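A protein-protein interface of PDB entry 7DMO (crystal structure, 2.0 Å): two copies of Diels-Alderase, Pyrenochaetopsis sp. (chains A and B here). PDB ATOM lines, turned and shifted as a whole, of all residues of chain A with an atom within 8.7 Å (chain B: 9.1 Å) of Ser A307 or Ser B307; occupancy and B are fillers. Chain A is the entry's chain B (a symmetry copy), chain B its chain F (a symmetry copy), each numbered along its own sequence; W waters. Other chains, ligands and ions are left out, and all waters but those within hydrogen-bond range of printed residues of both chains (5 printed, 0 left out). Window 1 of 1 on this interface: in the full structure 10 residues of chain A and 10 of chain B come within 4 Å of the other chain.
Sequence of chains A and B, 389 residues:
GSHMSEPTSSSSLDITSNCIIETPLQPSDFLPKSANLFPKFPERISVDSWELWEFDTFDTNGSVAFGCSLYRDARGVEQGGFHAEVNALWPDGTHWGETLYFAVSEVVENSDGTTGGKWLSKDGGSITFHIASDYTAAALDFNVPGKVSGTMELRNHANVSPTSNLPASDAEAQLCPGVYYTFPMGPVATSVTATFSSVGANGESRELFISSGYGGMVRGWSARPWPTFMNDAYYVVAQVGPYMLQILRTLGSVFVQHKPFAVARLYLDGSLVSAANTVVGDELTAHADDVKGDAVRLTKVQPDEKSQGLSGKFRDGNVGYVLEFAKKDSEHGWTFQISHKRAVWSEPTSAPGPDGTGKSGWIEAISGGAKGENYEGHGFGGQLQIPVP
Ser A307 touches four residues of chain B.
Gly A309 touches just one residue of chain B: Ser B307 (2.9 Å).
Of the printed residues of chain B, Gln A308 touches Ser B307 and Gln B308.
Of the printed residues of chain A, Ser B311 touches Pro A303 and Asp A304.
Glu A305 touches none of the printed residues of chain B.
Ala B365 touches none of the printed residues of chain A.
The nearest residue of chain B that does not touch Ser A307 is His B340 (4.8 Å).
The nearest residue of chain A that does not touch Ser B307 is His A340 (4.9 Å).
The nearest printed residue of chain B that does not touch Ser A311 is Glu B305 (5.4 Å).
Among the printed residues, merely in contact across the chains: Pro A303 with Leu B310 (3.4 Å), Asp A304 with Ser B311 (3.2 Å), Lys A306 with Leu B310 (3.7 Å), Ser A307 with Leu B310 (3.6 Å), Leu A310 with Pro B303 (3.4 Å), Leu A310 with Lys B306 (3.8 Å), Leu A310 with Ser B307 (3.6 Å) and Ser A311 with Asp B304 (3.2 Å).
OG of Ser A307 lies within hydrogen-bond range of NE2 of Gln B308 (3.2 Å).
The backbone carbonyl oxygen (O) of Ser B307 lies close to the backbone carbonyl oxygen (O) of Ser A307 (3.0 Å).
The backbone NH (N) of Ser A311 sits at hydrogen-bond distance from the backbone carbonyl oxygen (O) of Pro B303, at 2.9 Å.
N of Gly A309 lies within hydrogen-bond range of O of Ser B307 (2.9 Å).
OG of Ser B307 sits at hydrogen-bond distance from NE2 of Gln A308 (3.4 Å).
The side-chain amide oxygen (OE1) of Gln B308 sits close to the side-chain amide oxygen (OE1) of Gln A308.
The backbone carbonyl oxygen (O) of Ser A307 sits at hydrogen-bond distance from the backbone NH (N) of Gly B309.
The backbone NH (N) of Ser B311 is in hydrogen-bond range of the backbone carbonyl oxygen (O) of Pro A303.
Water W3 lies within hydrogen-bond range of the backbone carbonyl oxygen of Lys B341 (2.6 Å) and the side-chain hydroxyl of Ser A307 (3.1 Å).
Water W2 bridges O of Ser B311 and O of Asp A304.
Water W5 lies within hydrogen-bond range of the backbone carbonyl oxygen of Lys A341 (2.7 Å) and the side-chain hydroxyl of Ser B307 (3.0 Å).
The backbone NH of Leu B310 sits at hydrogen-bond distance from the backbone carbonyl oxygen of His B340 (2.9 Å).
O of Gln A308 sits at hydrogen-bond distance from OG of Ser A339 (3.1 Å).
O of His A340 is in hydrogen-bond range of N of Leu A310.
Pro A303 touches Leu B310, and with the chains exchanged Leu A310 touches Pro B303.
Pro A303 touches Ser B311, and with the chains exchanged Ser A311 touches Pro B303.
Positions printed for both chains: 301, 302, 303, 304, 305, 306, 307, 308, 309, 310, 311, 319, 339, 340, 341, 342, 343 and 362.
Printed residues of chain B that touch a printed residue of chain A: Pro B303, Asp B304, Lys B306, Ser B307, Gln B308, Gly B309, Leu B310 and Ser B311.
Hydrophobic or aromatic side chains of chain B that line the printed part of chain A: Pro B303 and Leu B310.
Of the 18 printed residues of chain A, 8 touch a printed residue of chain B.
Hydrophobic or aromatic side chains of chain A within 4 Å of the printed part of chain B: Pro A303 and Leu A310.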
ATOM      1  N   VAL A 301     -16.321 -18.193 -18.008  1.00  0.00           N
ATOM      2  CA  VAL A 301     -16.086 -16.791 -18.350  1.00  0.00           C
ATOM      3  C   VAL A 301     -15.213 -16.197 -17.254  1.00  0.00           C
ATOM      4  O   VAL A 301     -15.542 -16.313 -16.069  1.00  0.00           O
ATOM      5  CB  VAL A 301     -17.424 -16.020 -18.461  1.00  0.00           C
ATOM      6  CG1 VAL A 301     -17.193 -14.520 -18.653  1.00  0.00           C
ATOM      7  CG2 VAL A 301     -18.291 -16.571 -19.598  1.00  0.00           C
ATOM      8  N   GLN A 302     -14.121 -15.500 -17.652  1.00  0.00           N
ATOM      9  CA  GLN A 302     -13.164 -14.923 -16.722  1.00  0.00           C
ATOM     10  C   GLN A 302     -13.367 -13.419 -16.604  1.00  0.00           C
ATOM     11  O   GLN A 302     -13.862 -12.782 -17.540  1.00  0.00           O
ATOM     12  CB  GLN A 302     -11.726 -15.207 -17.193  1.00  0.00           C
ATOM     13  CG  GLN A 302     -11.463 -16.672 -17.453  1.00  0.00           C
ATOM     14  CD  GLN A 302     -11.646 -17.508 -16.200  1.00  0.00           C
ATOM     15  OE1 GLN A 302     -11.514 -17.001 -15.093  1.00  0.00           O
ATOM     16  NE2 GLN A 302     -11.949 -18.797 -16.371  1.00  0.00           N
ATOM     17  N   PRO A 303     -12.982 -12.810 -15.474  1.00  0.00           N
ATOM     18  CA  PRO A 303     -13.210 -11.362 -15.309  1.00  0.00           C
ATOM     19  C   PRO A 303     -12.399 -10.492 -16.265  1.00  0.00           C
ATOM     20  O   PRO A 303     -12.697  -9.296 -16.378  1.00  0.00           O
ATOM     21  CB  PRO A 303     -12.807 -11.098 -13.848  1.00  0.00           C
ATOM     22  CG  PRO A 303     -11.886 -12.229 -13.479  1.00  0.00           C
ATOM     23  CD  PRO A 303     -12.273 -13.414 -14.330  1.00  0.00           C
ATOM     24  N   ASP A 304     -11.377 -11.021 -16.944  1.00  0.00           N
ATOM     25  CA  ASP A 304     -10.710 -10.190 -17.944  1.00  0.00           C
ATOM     26  C   ASP A 304     -11.478 -10.145 -19.258  1.00  0.00           C
ATOM     27  O   ASP A 304     -11.095  -9.376 -20.154  1.00  0.00           O
ATOM     28  CB  ASP A 304      -9.291 -10.686 -18.201  1.00  0.00           C
ATOM     29  CG  ASP A 304      -9.277 -12.116 -18.732  1.00  0.00           C
ATOM     30  OD1 ASP A 304      -9.406 -13.048 -17.909  1.00  0.00           O
ATOM     31  OD2 ASP A 304      -9.160 -12.300 -19.959  1.00  0.00           O
ATOM     32  N   GLU A 305     -12.566 -10.926 -19.371  1.00  0.00           N
ATOM     33  CA  GLU A 305     -13.405 -10.988 -20.564  1.00  0.00           C
ATOM     34  C   GLU A 305     -14.752 -10.320 -20.394  1.00  0.00           C
ATOM     35  O   GLU A 305     -15.281  -9.779 -21.364  1.00  0.00           O
ATOM     36  CB  GLU A 305     -13.657 -12.448 -20.973  1.00  0.00           C
ATOM     37  CG  GLU A 305     -12.396 -13.269 -20.971  1.00  0.00           C
ATOM     38  CD  GLU A 305     -12.649 -14.756 -21.049  1.00  0.00           C
ATOM     39  OE1 GLU A 305     -13.663 -15.238 -20.509  1.00  0.00           O
ATOM     40  OE2 GLU A 305     -11.799 -15.445 -21.638  1.00  0.00           O
ATOM     41  N   LYS A 306     -15.331 -10.366 -19.197  1.00  0.00           N
ATOM     42  CA  LYS A 306     -16.666  -9.833 -18.969  1.00  0.00           C
ATOM     43  C   LYS A 306     -16.660  -9.098 -17.639  1.00  0.00           C
ATOM     44  O   LYS A 306     -16.161  -9.631 -16.641  1.00  0.00           O
ATOM     45  CB  LYS A 306     -17.711 -10.952 -18.947  1.00  0.00           C
ATOM     46  CG  LYS A 306     -19.112 -10.442 -18.700  1.00  0.00           C
ATOM     47  CD  LYS A 306     -20.157 -11.494 -18.993  1.00  0.00           C
ATOM     48  CE  LYS A 306     -21.536 -10.988 -18.560  1.00  0.00           C
ATOM     49  NZ  LYS A 306     -21.887  -9.745 -19.320  1.00  0.00           N
ATOM     50  N   SER A 307     -17.205  -7.874 -17.626  1.00  0.00           N
ATOM     51  CA  SER A 307     -17.115  -7.046 -16.430  1.00  0.00           C
ATOM     52  C   SER A 307     -18.137  -7.422 -15.369  1.00  0.00           C
ATOM     53  O   SER A 307     -17.887  -7.204 -14.183  1.00  0.00           O
ATOM     54  CB  SER A 307     -17.301  -5.571 -16.782  1.00  0.00           C
ATOM     55  OG  SER A 307     -18.505  -5.382 -17.504  1.00  0.00           O
ATOM     56  N   GLN A 308     -19.293  -7.947 -15.757  1.00  0.00           N
ATOM     57  CA  GLN A 308     -20.375  -8.169 -14.810  1.00  0.00           C
ATOM     58  C   GLN A 308     -20.333  -9.608 -14.314  1.00  0.00           C
ATOM     59  O   GLN A 308     -20.306 -10.538 -15.120  1.00  0.00           O
ATOM     60  CB  GLN A 308     -21.722  -7.859 -15.470  1.00  0.00           C
ATOM     61  CG  GLN A 308     -22.922  -7.999 -14.551  1.00  0.00           C
ATOM     62  CD  GLN A 308     -22.987  -6.890 -13.505  1.00  0.00           C
ATOM     63  OE1 GLN A 308     -23.526  -5.805 -13.755  1.00  0.00           O
ATOM     64  NE2 GLN A 308     -22.452  -7.170 -12.315  1.00  0.00           N
ATOM     65  N   GLY A 309     -20.336  -9.783 -12.992  1.00  0.00           N
ATOM     66  CA  GLY A 309     -20.321 -11.108 -12.395  1.00  0.00           C
ATOM     67  C   GLY A 309     -19.340 -11.267 -11.244  1.00  0.00           C
ATOM     68  O   GLY A 309     -18.191 -10.830 -11.351  1.00  0.00           O
ATOM     69  N   LEU A 310     -19.781 -11.888 -10.144  1.00  0.00           N
ATOM     70  CA  LEU A 310     -18.884 -12.250  -9.046  1.00  0.00           C
ATOM     71  C   LEU A 310     -18.064 -13.490  -9.357  1.00  0.00           C
ATOM     72  O   LEU A 310     -18.462 -14.351 -10.154  1.00  0.00           O
ATOM     73  CB  LEU A 310     -19.663 -12.527  -7.762  1.00  0.00           C
ATOM     74  CG  LEU A 310     -20.377 -11.343  -7.140  1.00  0.00           C
ATOM     75  CD1 LEU A 310     -21.462 -11.844  -6.170  1.00  0.00           C
ATOM     76  CD2 LEU A 310     -19.345 -10.477  -6.415  1.00  0.00           C
ATOM     77  N   SER A 311     -16.911 -13.575  -8.701  1.00  0.00           N
ATOM     78  CA  SER A 311     -16.092 -14.773  -8.622  1.00  0.00           C
ATOM     79  C   SER A 311     -16.294 -15.450  -7.266  1.00  0.00           C
ATOM     80  O   SER A 311     -16.605 -14.794  -6.266  1.00  0.00           O
ATOM     81  CB  SER A 311     -14.612 -14.405  -8.816  1.00  0.00           C
ATOM     82  OG  SER A 311     -13.761 -15.402  -8.294  1.00  0.00           O
ATOM     83  N   VAL A 319     -16.222 -15.788 -13.522  1.00  0.00           N
ATOM     84  CA  VAL A 319     -17.334 -14.943 -13.106  1.00  0.00           C
ATOM     85  C   VAL A 319     -18.630 -15.376 -13.768  1.00  0.00           C
ATOM     86  O   VAL A 319     -19.632 -14.671 -13.666  1.00  0.00           O
ATOM     87  CB  VAL A 319     -17.072 -13.446 -13.372  1.00  0.00           C
ATOM     88  CG1 VAL A 319     -15.883 -12.933 -12.561  1.00  0.00           C
ATOM     89  CG2 VAL A 319     -16.924 -13.171 -14.874  1.00  0.00           C
ATOM     90  N   SER A 339     -24.157 -15.284 -15.475  1.00  0.00           N
ATOM     91  CA  SER A 339     -23.307 -14.387 -14.690  1.00  0.00           C
ATOM     92  C   SER A 339     -23.569 -14.623 -13.207  1.00  0.00           C
ATOM     93  O   SER A 339     -24.726 -14.683 -12.797  1.00  0.00           O
ATOM     94  CB  SER A 339     -23.592 -12.910 -15.062  1.00  0.00           C
ATOM     95  OG  SER A 339     -22.879 -12.065 -14.204  1.00  0.00           O
ATOM     96  N   HIS A 340     -22.514 -14.731 -12.385  1.00  0.00           N
ATOM     97  CA  HIS A 340     -22.730 -14.976 -10.955  1.00  0.00           C
ATOM     98  C   HIS A 340     -23.200 -13.685 -10.282  1.00  0.00           C
ATOM     99  O   HIS A 340     -22.414 -12.754 -10.093  1.00  0.00           O
ATOM    100  CB  HIS A 340     -21.463 -15.502 -10.284  1.00  0.00           C
ATOM    101  CG  HIS A 340     -20.951 -16.775 -10.878  1.00  0.00           C
ATOM    102  ND1 HIS A 340     -21.784 -17.813 -11.257  1.00  0.00           N
ATOM    103  CD2 HIS A 340     -19.691 -17.173 -11.168  1.00  0.00           C
ATOM    104  CE1 HIS A 340     -21.052 -18.803 -11.733  1.00  0.00           C
ATOM    105  NE2 HIS A 340     -19.781 -18.440 -11.696  1.00  0.00           N
ATOM    106  N   LYS A 341     -24.470 -13.649  -9.878  1.00  0.00           N
ATOM    107  CA  LYS A 341     -25.092 -12.428  -9.383  1.00  0.00           C
ATOM    108  C   LYS A 341     -25.039 -12.285  -7.859  1.00  0.00           C
ATOM    109  O   LYS A 341     -24.778 -11.186  -7.353  1.00  0.00           O
ATOM    110  CB  LYS A 341     -26.552 -12.360  -9.848  1.00  0.00           C
ATOM    111  CG  LYS A 341     -27.243 -11.003  -9.556  1.00  0.00           C
ATOM    112  CD  LYS A 341     -28.686 -10.989 -10.111  1.00  0.00           C
ATOM    113  CE  LYS A 341     -29.362  -9.650  -9.847  1.00  0.00           C
ATOM    114  NZ  LYS A 341     -30.818  -9.696 -10.176  1.00  0.00           N
ATOM    115  N   ARG A 342     -25.314 -13.350  -7.115  1.00  0.00           N
ATOM    116  CA  ARG A 342     -25.375 -13.288  -5.658  1.00  0.00           C
ATOM    117  C   ARG A 342     -24.762 -14.548  -5.066  1.00  0.00           C
ATOM    118  O   ARG A 342     -25.073 -15.659  -5.514  1.00  0.00           O
ATOM    119  CB  ARG A 342     -26.826 -13.146  -5.164  1.00  0.00           C
ATOM    120  CG  ARG A 342     -27.683 -12.183  -5.989  1.00  0.00           C
ATOM    121  CD  ARG A 342     -29.087 -12.080  -5.440  1.00  0.00           C
ATOM    122  NE  ARG A 342     -29.062 -11.544  -4.086  1.00  0.00           N
ATOM    123  CZ  ARG A 342     -30.014 -11.749  -3.176  1.00  0.00           C
ATOM    124  NH1 ARG A 342     -31.092 -12.476  -3.467  1.00  0.00           N
ATOM    125  NH2 ARG A 342     -29.881 -11.225  -1.969  1.00  0.00           N
ATOM    126  N   ALA A 343     -23.898 -14.369  -4.062  1.00  0.00           N
ATOM    127  CA  ALA A 343     -23.221 -15.506  -3.395  1.00  0.00           C
ATOM    128  C   ALA A 343     -24.163 -16.138  -2.362  1.00  0.00           C
ATOM    129  O   ALA A 343     -24.718 -15.393  -1.531  1.00  0.00           O
ATOM    130  CB  ALA A 343     -21.937 -15.037  -2.757  1.00  0.00           C
ATOM    131  N   TRP A 362     -24.718 -20.033  -5.962  1.00  0.00           N
ATOM    132  CA  TRP A 362     -25.006 -18.795  -6.702  1.00  0.00           C
ATOM    133  C   TRP A 362     -26.492 -18.577  -7.022  1.00  0.00           C
ATOM    134  O   TRP A 362     -27.190 -19.532  -7.317  1.00  0.00           O
ATOM    135  CB  TRP A 362     -24.270 -18.870  -8.049  1.00  0.00           C
ATOM    136  CG  TRP A 362     -22.776 -18.947  -8.050  1.00  0.00           C
ATOM    137  CD1 TRP A 362     -22.002 -19.945  -8.546  1.00  0.00           C
ATOM    138  CD2 TRP A 362     -21.874 -17.969  -7.530  1.00  0.00           C
ATOM    139  NE1 TRP A 362     -20.685 -19.652  -8.395  1.00  0.00           N
ATOM    140  CE2 TRP A 362     -20.573 -18.438  -7.781  1.00  0.00           C
ATOM    141  CE3 TRP A 362     -22.033 -16.737  -6.907  1.00  0.00           C
ATOM    142  CZ2 TRP A 362     -19.448 -17.735  -7.381  1.00  0.00           C
ATOM    143  CZ3 TRP A 362     -20.925 -16.027  -6.536  1.00  0.00           C
ATOM    144  CH2 TRP A 362     -19.650 -16.529  -6.770  1.00  0.00           C
ATOM    145  N   VAL B 301      -9.646  -4.098  -5.099  1.00  0.00           N
ATOM    146  CA  VAL B 301     -10.911  -4.824  -5.034  1.00  0.00           C
ATOM    147  C   VAL B 301     -10.798  -6.088  -5.873  1.00  0.00           C
ATOM    148  O   VAL B 301     -10.336  -6.043  -7.025  1.00  0.00           O
ATOM    149  CB  VAL B 301     -12.080  -3.956  -5.530  1.00  0.00           C
ATOM    150  CG1 VAL B 301     -13.397  -4.754  -5.547  1.00  0.00           C
ATOM    151  CG2 VAL B 301     -12.216  -2.714  -4.686  1.00  0.00           C
ATOM    152  N   GLN B 302     -11.253  -7.212  -5.313  1.00  0.00           N
ATOM    153  CA  GLN B 302     -11.232  -8.484  -6.025  1.00  0.00           C
ATOM    154  C   GLN B 302     -12.619  -8.824  -6.559  1.00  0.00           C
ATOM    155  O   GLN B 302     -13.633  -8.379  -6.015  1.00  0.00           O
ATOM    156  CB  GLN B 302     -10.743  -9.604  -5.094  1.00  0.00           C
ATOM    157  CG  GLN B 302      -9.346  -9.361  -4.524  1.00  0.00           C
ATOM    158  CD  GLN B 302      -8.301  -9.039  -5.614  1.00  0.00           C
ATOM    159  OE1 GLN B 302      -8.362  -9.558  -6.738  1.00  0.00           O
ATOM    160  NE2 GLN B 302      -7.335  -8.193  -5.269  1.00  0.00           N
ATOM    161  N   PRO B 303     -12.706  -9.634  -7.621  1.00  0.00           N
ATOM    162  CA  PRO B 303     -14.028  -9.967  -8.187  1.00  0.00           C
ATOM    163  C   PRO B 303     -14.853 -10.876  -7.301  1.00  0.00           C
ATOM    164  O   PRO B 303     -16.036 -11.093  -7.597  1.00  0.00           O
ATOM    165  CB  PRO B 303     -13.677 -10.647  -9.518  1.00  0.00           C
ATOM    166  CG  PRO B 303     -12.325 -11.183  -9.324  1.00  0.00           C
ATOM    167  CD  PRO B 303     -11.609 -10.256  -8.380  1.00  0.00           C
ATOM    168  N   ASP B 304     -14.286 -11.417  -6.220  1.00  0.00           N
ATOM    169  CA  ASP B 304     -15.140 -12.104  -5.255  1.00  0.00           C
ATOM    170  C   ASP B 304     -15.767 -11.143  -4.268  1.00  0.00           C
ATOM    171  O   ASP B 304     -16.603 -11.566  -3.471  1.00  0.00           O
ATOM    172  CB  ASP B 304     -14.353 -13.165  -4.486  1.00  0.00           C
ATOM    173  CG  ASP B 304     -13.247 -12.556  -3.659  1.00  0.00           C
ATOM    174  OD1 ASP B 304     -12.171 -12.294  -4.226  1.00  0.00           O
ATOM    175  OD2 ASP B 304     -13.480 -12.290  -2.471  1.00  0.00           O
ATOM    176  N   GLU B 305     -15.377  -9.868  -4.307  1.00  0.00           N
ATOM    177  CA  GLU B 305     -15.923  -8.823  -3.459  1.00  0.00           C
ATOM    178  C   GLU B 305     -16.910  -7.928  -4.191  1.00  0.00           C
ATOM    179  O   GLU B 305     -17.875  -7.453  -3.598  1.00  0.00           O
ATOM    180  CB  GLU B 305     -14.784  -7.945  -2.897  1.00  0.00           C
ATOM    181  CG  GLU B 305     -13.816  -8.697  -2.001  1.00  0.00           C
ATOM    182  CD  GLU B 305     -12.444  -8.000  -1.800  1.00  0.00           C
ATOM    183  OE1 GLU B 305     -12.030  -7.129  -2.609  1.00  0.00           O
ATOM    184  OE2 GLU B 305     -11.778  -8.340  -0.801  1.00  0.00           O
ATOM    185  N   LYS B 306     -16.676  -7.641  -5.459  1.00  0.00           N
ATOM    186  CA  LYS B 306     -17.496  -6.667  -6.161  1.00  0.00           C
ATOM    187  C   LYS B 306     -17.813  -7.227  -7.540  1.00  0.00           C
ATOM    188  O   LYS B 306     -16.914  -7.716  -8.235  1.00  0.00           O
ATOM    189  CB  LYS B 306     -16.774  -5.321  -6.247  1.00  0.00           C
ATOM    190  CG  LYS B 306     -17.600  -4.167  -6.818  1.00  0.00           C
ATOM    191  CD  LYS B 306     -17.072  -2.814  -6.350  1.00  0.00           C
ATOM    192  CE  LYS B 306     -17.388  -1.688  -7.367  1.00  0.00           C
ATOM    193  NZ  LYS B 306     -18.819  -1.698  -7.827  1.00  0.00           N
ATOM    194  N   SER B 307     -19.094  -7.179  -7.925  1.00  0.00           N
ATOM    195  CA  SER B 307     -19.499  -7.858  -9.147  1.00  0.00           C
ATOM    196  C   SER B 307     -19.157  -7.077 -10.408  1.00  0.00           C
ATOM    197  O   SER B 307     -18.983  -7.685 -11.465  1.00  0.00           O
ATOM    198  CB  SER B 307     -21.001  -8.163  -9.129  1.00  0.00           C
ATOM    199  OG  SER B 307     -21.785  -6.982  -9.025  1.00  0.00           O
ATOM    200  N   GLN B 308     -19.071  -5.752 -10.354  1.00  0.00           N
ATOM    201  CA  GLN B 308     -18.806  -4.983 -11.566  1.00  0.00           C
ATOM    202  C   GLN B 308     -17.339  -4.571 -11.664  1.00  0.00           C
ATOM    203  O   GLN B 308     -16.741  -4.144 -10.677  1.00  0.00           O
ATOM    204  CB  GLN B 308     -19.698  -3.752 -11.633  1.00  0.00           C
ATOM    205  CG  GLN B 308     -19.591  -3.037 -12.966  1.00  0.00           C
ATOM    206  CD  GLN B 308     -20.419  -3.715 -14.058  1.00  0.00           C
ATOM    207  OE1 GLN B 308     -21.404  -4.423 -13.775  1.00  0.00           O
ATOM    208  NE2 GLN B 308     -20.006  -3.521 -15.317  1.00  0.00           N
ATOM    209  N   GLY B 309     -16.768  -4.710 -12.864  1.00  0.00           N
ATOM    210  CA  GLY B 309     -15.387  -4.337 -13.138  1.00  0.00           C
ATOM    211  C   GLY B 309     -14.584  -5.420 -13.842  1.00  0.00           C
ATOM    212  O   GLY B 309     -14.727  -6.592 -13.516  1.00  0.00           O
ATOM    213  N   LEU B 310     -13.761  -5.047 -14.824  1.00  0.00           N
ATOM    214  CA  LEU B 310     -12.880  -5.992 -15.492  1.00  0.00           C
ATOM    215  C   LEU B 310     -11.592  -6.174 -14.704  1.00  0.00           C
ATOM    216  O   LEU B 310     -11.161  -5.285 -13.969  1.00  0.00           O
ATOM    217  CB  LEU B 310     -12.507  -5.496 -16.893  1.00  0.00           C
ATOM    218  CG  LEU B 310     -13.622  -5.434 -17.936  1.00  0.00           C
ATOM    219  CD1 LEU B 310     -13.263  -4.439 -19.061  1.00  0.00           C
ATOM    220  CD2 LEU B 310     -13.860  -6.859 -18.479  1.00  0.00           C
ATOM    221  N   SER B 311     -10.964  -7.327 -14.899  1.00  0.00           N
ATOM    222  CA  SER B 311      -9.603  -7.595 -14.468  1.00  0.00           C
ATOM    223  C   SER B 311      -8.654  -7.447 -15.654  1.00  0.00           C
ATOM    224  O   SER B 311      -9.035  -7.689 -16.798  1.00  0.00           O
ATOM    225  CB  SER B 311      -9.512  -9.019 -13.910  1.00  0.00           C
ATOM    226  OG  SER B 311      -8.180  -9.493 -13.928  1.00  0.00           O
ATOM    227  N   VAL B 319     -10.294  -5.957  -9.862  1.00  0.00           N
ATOM    228  CA  VAL B 319     -11.314  -5.401 -10.747  1.00  0.00           C
ATOM    229  C   VAL B 319     -11.579  -3.934 -10.429  1.00  0.00           C
ATOM    230  O   VAL B 319     -12.527  -3.351 -10.960  1.00  0.00           O
ATOM    231  CB  VAL B 319     -12.631  -6.210 -10.700  1.00  0.00           C
ATOM    232  CG1 VAL B 319     -12.441  -7.632 -11.256  1.00  0.00           C
ATOM    233  CG2 VAL B 319     -13.230  -6.245  -9.283  1.00  0.00           C
ATOM    234  N   SER B 339     -13.928   1.144 -10.541  1.00  0.00           N
ATOM    235  CA  SER B 339     -14.030  -0.150 -11.222  1.00  0.00           C
ATOM    236  C   SER B 339     -13.541  -0.018 -12.654  1.00  0.00           C
ATOM    237  O   SER B 339     -13.793   0.992 -13.311  1.00  0.00           O
ATOM    238  CB  SER B 339     -15.472  -0.703 -11.244  1.00  0.00           C
ATOM    239  OG  SER B 339     -16.316   0.226 -11.879  1.00  0.00           O
ATOM    240  N   HIS B 340     -12.860  -1.056 -13.142  1.00  0.00           N
ATOM    241  CA  HIS B 340     -12.276  -1.034 -14.474  1.00  0.00           C
ATOM    242  C   HIS B 340     -13.383  -1.235 -15.510  1.00  0.00           C
ATOM    243  O   HIS B 340     -14.001  -2.295 -15.553  1.00  0.00           O
ATOM    244  CB  HIS B 340     -11.206  -2.117 -14.576  1.00  0.00           C
ATOM    245  CG  HIS B 340     -10.127  -1.991 -13.542  1.00  0.00           C
ATOM    246  ND1 HIS B 340      -9.594  -0.772 -13.180  1.00  0.00           N
ATOM    247  CD2 HIS B 340      -9.479  -2.924 -12.800  1.00  0.00           C
ATOM    248  CE1 HIS B 340      -8.663  -0.957 -12.256  1.00  0.00           C
ATOM    249  NE2 HIS B 340      -8.568  -2.254 -12.013  1.00  0.00           N
ATOM    250  N   LYS B 341     -13.641  -0.224 -16.340  1.00  0.00           N
ATOM    251  CA  LYS B 341     -14.805  -0.254 -17.228  1.00  0.00           C
ATOM    252  C   LYS B 341     -14.443  -0.672 -18.649  1.00  0.00           C
ATOM    253  O   LYS B 341     -15.139  -1.495 -19.250  1.00  0.00           O
ATOM    254  CB  LYS B 341     -15.491   1.128 -17.231  1.00  0.00           C
ATOM    255  CG  LYS B 341     -16.797   1.240 -18.039  1.00  0.00           C
ATOM    256  CD  LYS B 341     -17.027   2.727 -18.482  1.00  0.00           C
ATOM    257  CE  LYS B 341     -18.298   2.870 -19.347  1.00  0.00           C
ATOM    258  NZ  LYS B 341     -18.754   4.291 -19.485  1.00  0.00           N
ATOM    259  N   ARG B 342     -13.372  -0.105 -19.206  1.00  0.00           N
ATOM    260  CA  ARG B 342     -12.950  -0.398 -20.566  1.00  0.00           C
ATOM    261  C   ARG B 342     -11.435  -0.525 -20.621  1.00  0.00           C
ATOM    262  O   ARG B 342     -10.709   0.344 -20.122  1.00  0.00           O
ATOM    263  CB  ARG B 342     -13.395   0.686 -21.541  1.00  0.00           C
ATOM    264  CG  ARG B 342     -14.769   1.274 -21.298  1.00  0.00           C
ATOM    265  CD  ARG B 342     -15.211   2.038 -22.520  1.00  0.00           C
ATOM    266  NE  ARG B 342     -15.548   1.125 -23.616  1.00  0.00           N
ATOM    267  CZ  ARG B 342     -15.465   1.443 -24.908  1.00  0.00           C
ATOM    268  NH1 ARG B 342     -15.051   2.655 -25.281  1.00  0.00           N
ATOM    269  NH2 ARG B 342     -15.792   0.542 -25.829  1.00  0.00           N
ATOM    270  N   ALA B 343     -10.964  -1.620 -21.226  1.00  0.00           N
ATOM    271  CA  ALA B 343      -9.512  -1.891 -21.352  1.00  0.00           C
ATOM    272  C   ALA B 343      -8.920  -1.035 -22.477  1.00  0.00           C
ATOM    273  O   ALA B 343      -9.522  -0.990 -23.569  1.00  0.00           O
ATOM    274  CB  ALA B 343      -9.283  -3.362 -21.597  1.00  0.00           C
ATOM    275  N   TRP B 362      -6.857   1.727 -18.493  1.00  0.00           N
ATOM    276  CA  TRP B 362      -8.301   1.631 -18.223  1.00  0.00           C
ATOM    277  C   TRP B 362      -9.017   2.969 -18.393  1.00  0.00           C
ATOM    278  O   TRP B 362      -8.436   3.983 -18.132  1.00  0.00           O
ATOM    279  CB  TRP B 362      -8.505   1.252 -16.758  1.00  0.00           C
ATOM    280  CG  TRP B 362      -7.926  -0.032 -16.263  1.00  0.00           C
ATOM    281  CD1 TRP B 362      -6.974  -0.202 -15.310  1.00  0.00           C
ATOM    282  CD2 TRP B 362      -8.302  -1.341 -16.684  1.00  0.00           C
ATOM    283  NE1 TRP B 362      -6.740  -1.525 -15.091  1.00  0.00           N
ATOM    284  CE2 TRP B 362      -7.539  -2.250 -15.925  1.00  0.00           C
ATOM    285  CE3 TRP B 362      -9.217  -1.823 -17.617  1.00  0.00           C
ATOM    286  CZ2 TRP B 362      -7.638  -3.623 -16.099  1.00  0.00           C
ATOM    287  CZ3 TRP B 362      -9.325  -3.180 -17.773  1.00  0.00           C
ATOM    288  CH2 TRP B 362      -8.554  -4.061 -17.022  1.00  0.00           C
ATOM    289  N   ALA B 365     -14.679   3.549 -14.162  1.00  0.00           N
ATOM    290  CA  ALA B 365     -16.011   3.966 -13.690  1.00  0.00           C
ATOM    291  C   ALA B 365     -15.808   4.261 -12.192  1.00  0.00           C
ATOM    292  O   ALA B 365     -15.344   3.393 -11.500  1.00  0.00           O
ATOM    293  CB  ALA B 365     -17.020   2.893 -13.966  1.00  0.00           C
HETATM  294  O   HOH W   1     -23.631  -9.141 -10.942  1.00  0.00           O
HETATM  295  O   HOH W   2      -8.969  -6.782 -19.276  1.00  0.00           O
HETATM  296  O   HOH W   3     -17.343  -2.607 -18.399  1.00  0.00           O
HETATM  297  O   HOH W   4     -18.221 -14.309  -4.319  1.00  0.00           O
HETATM  298  O   HOH W   5     -24.046  -8.830  -8.524  1.00  0.00           O
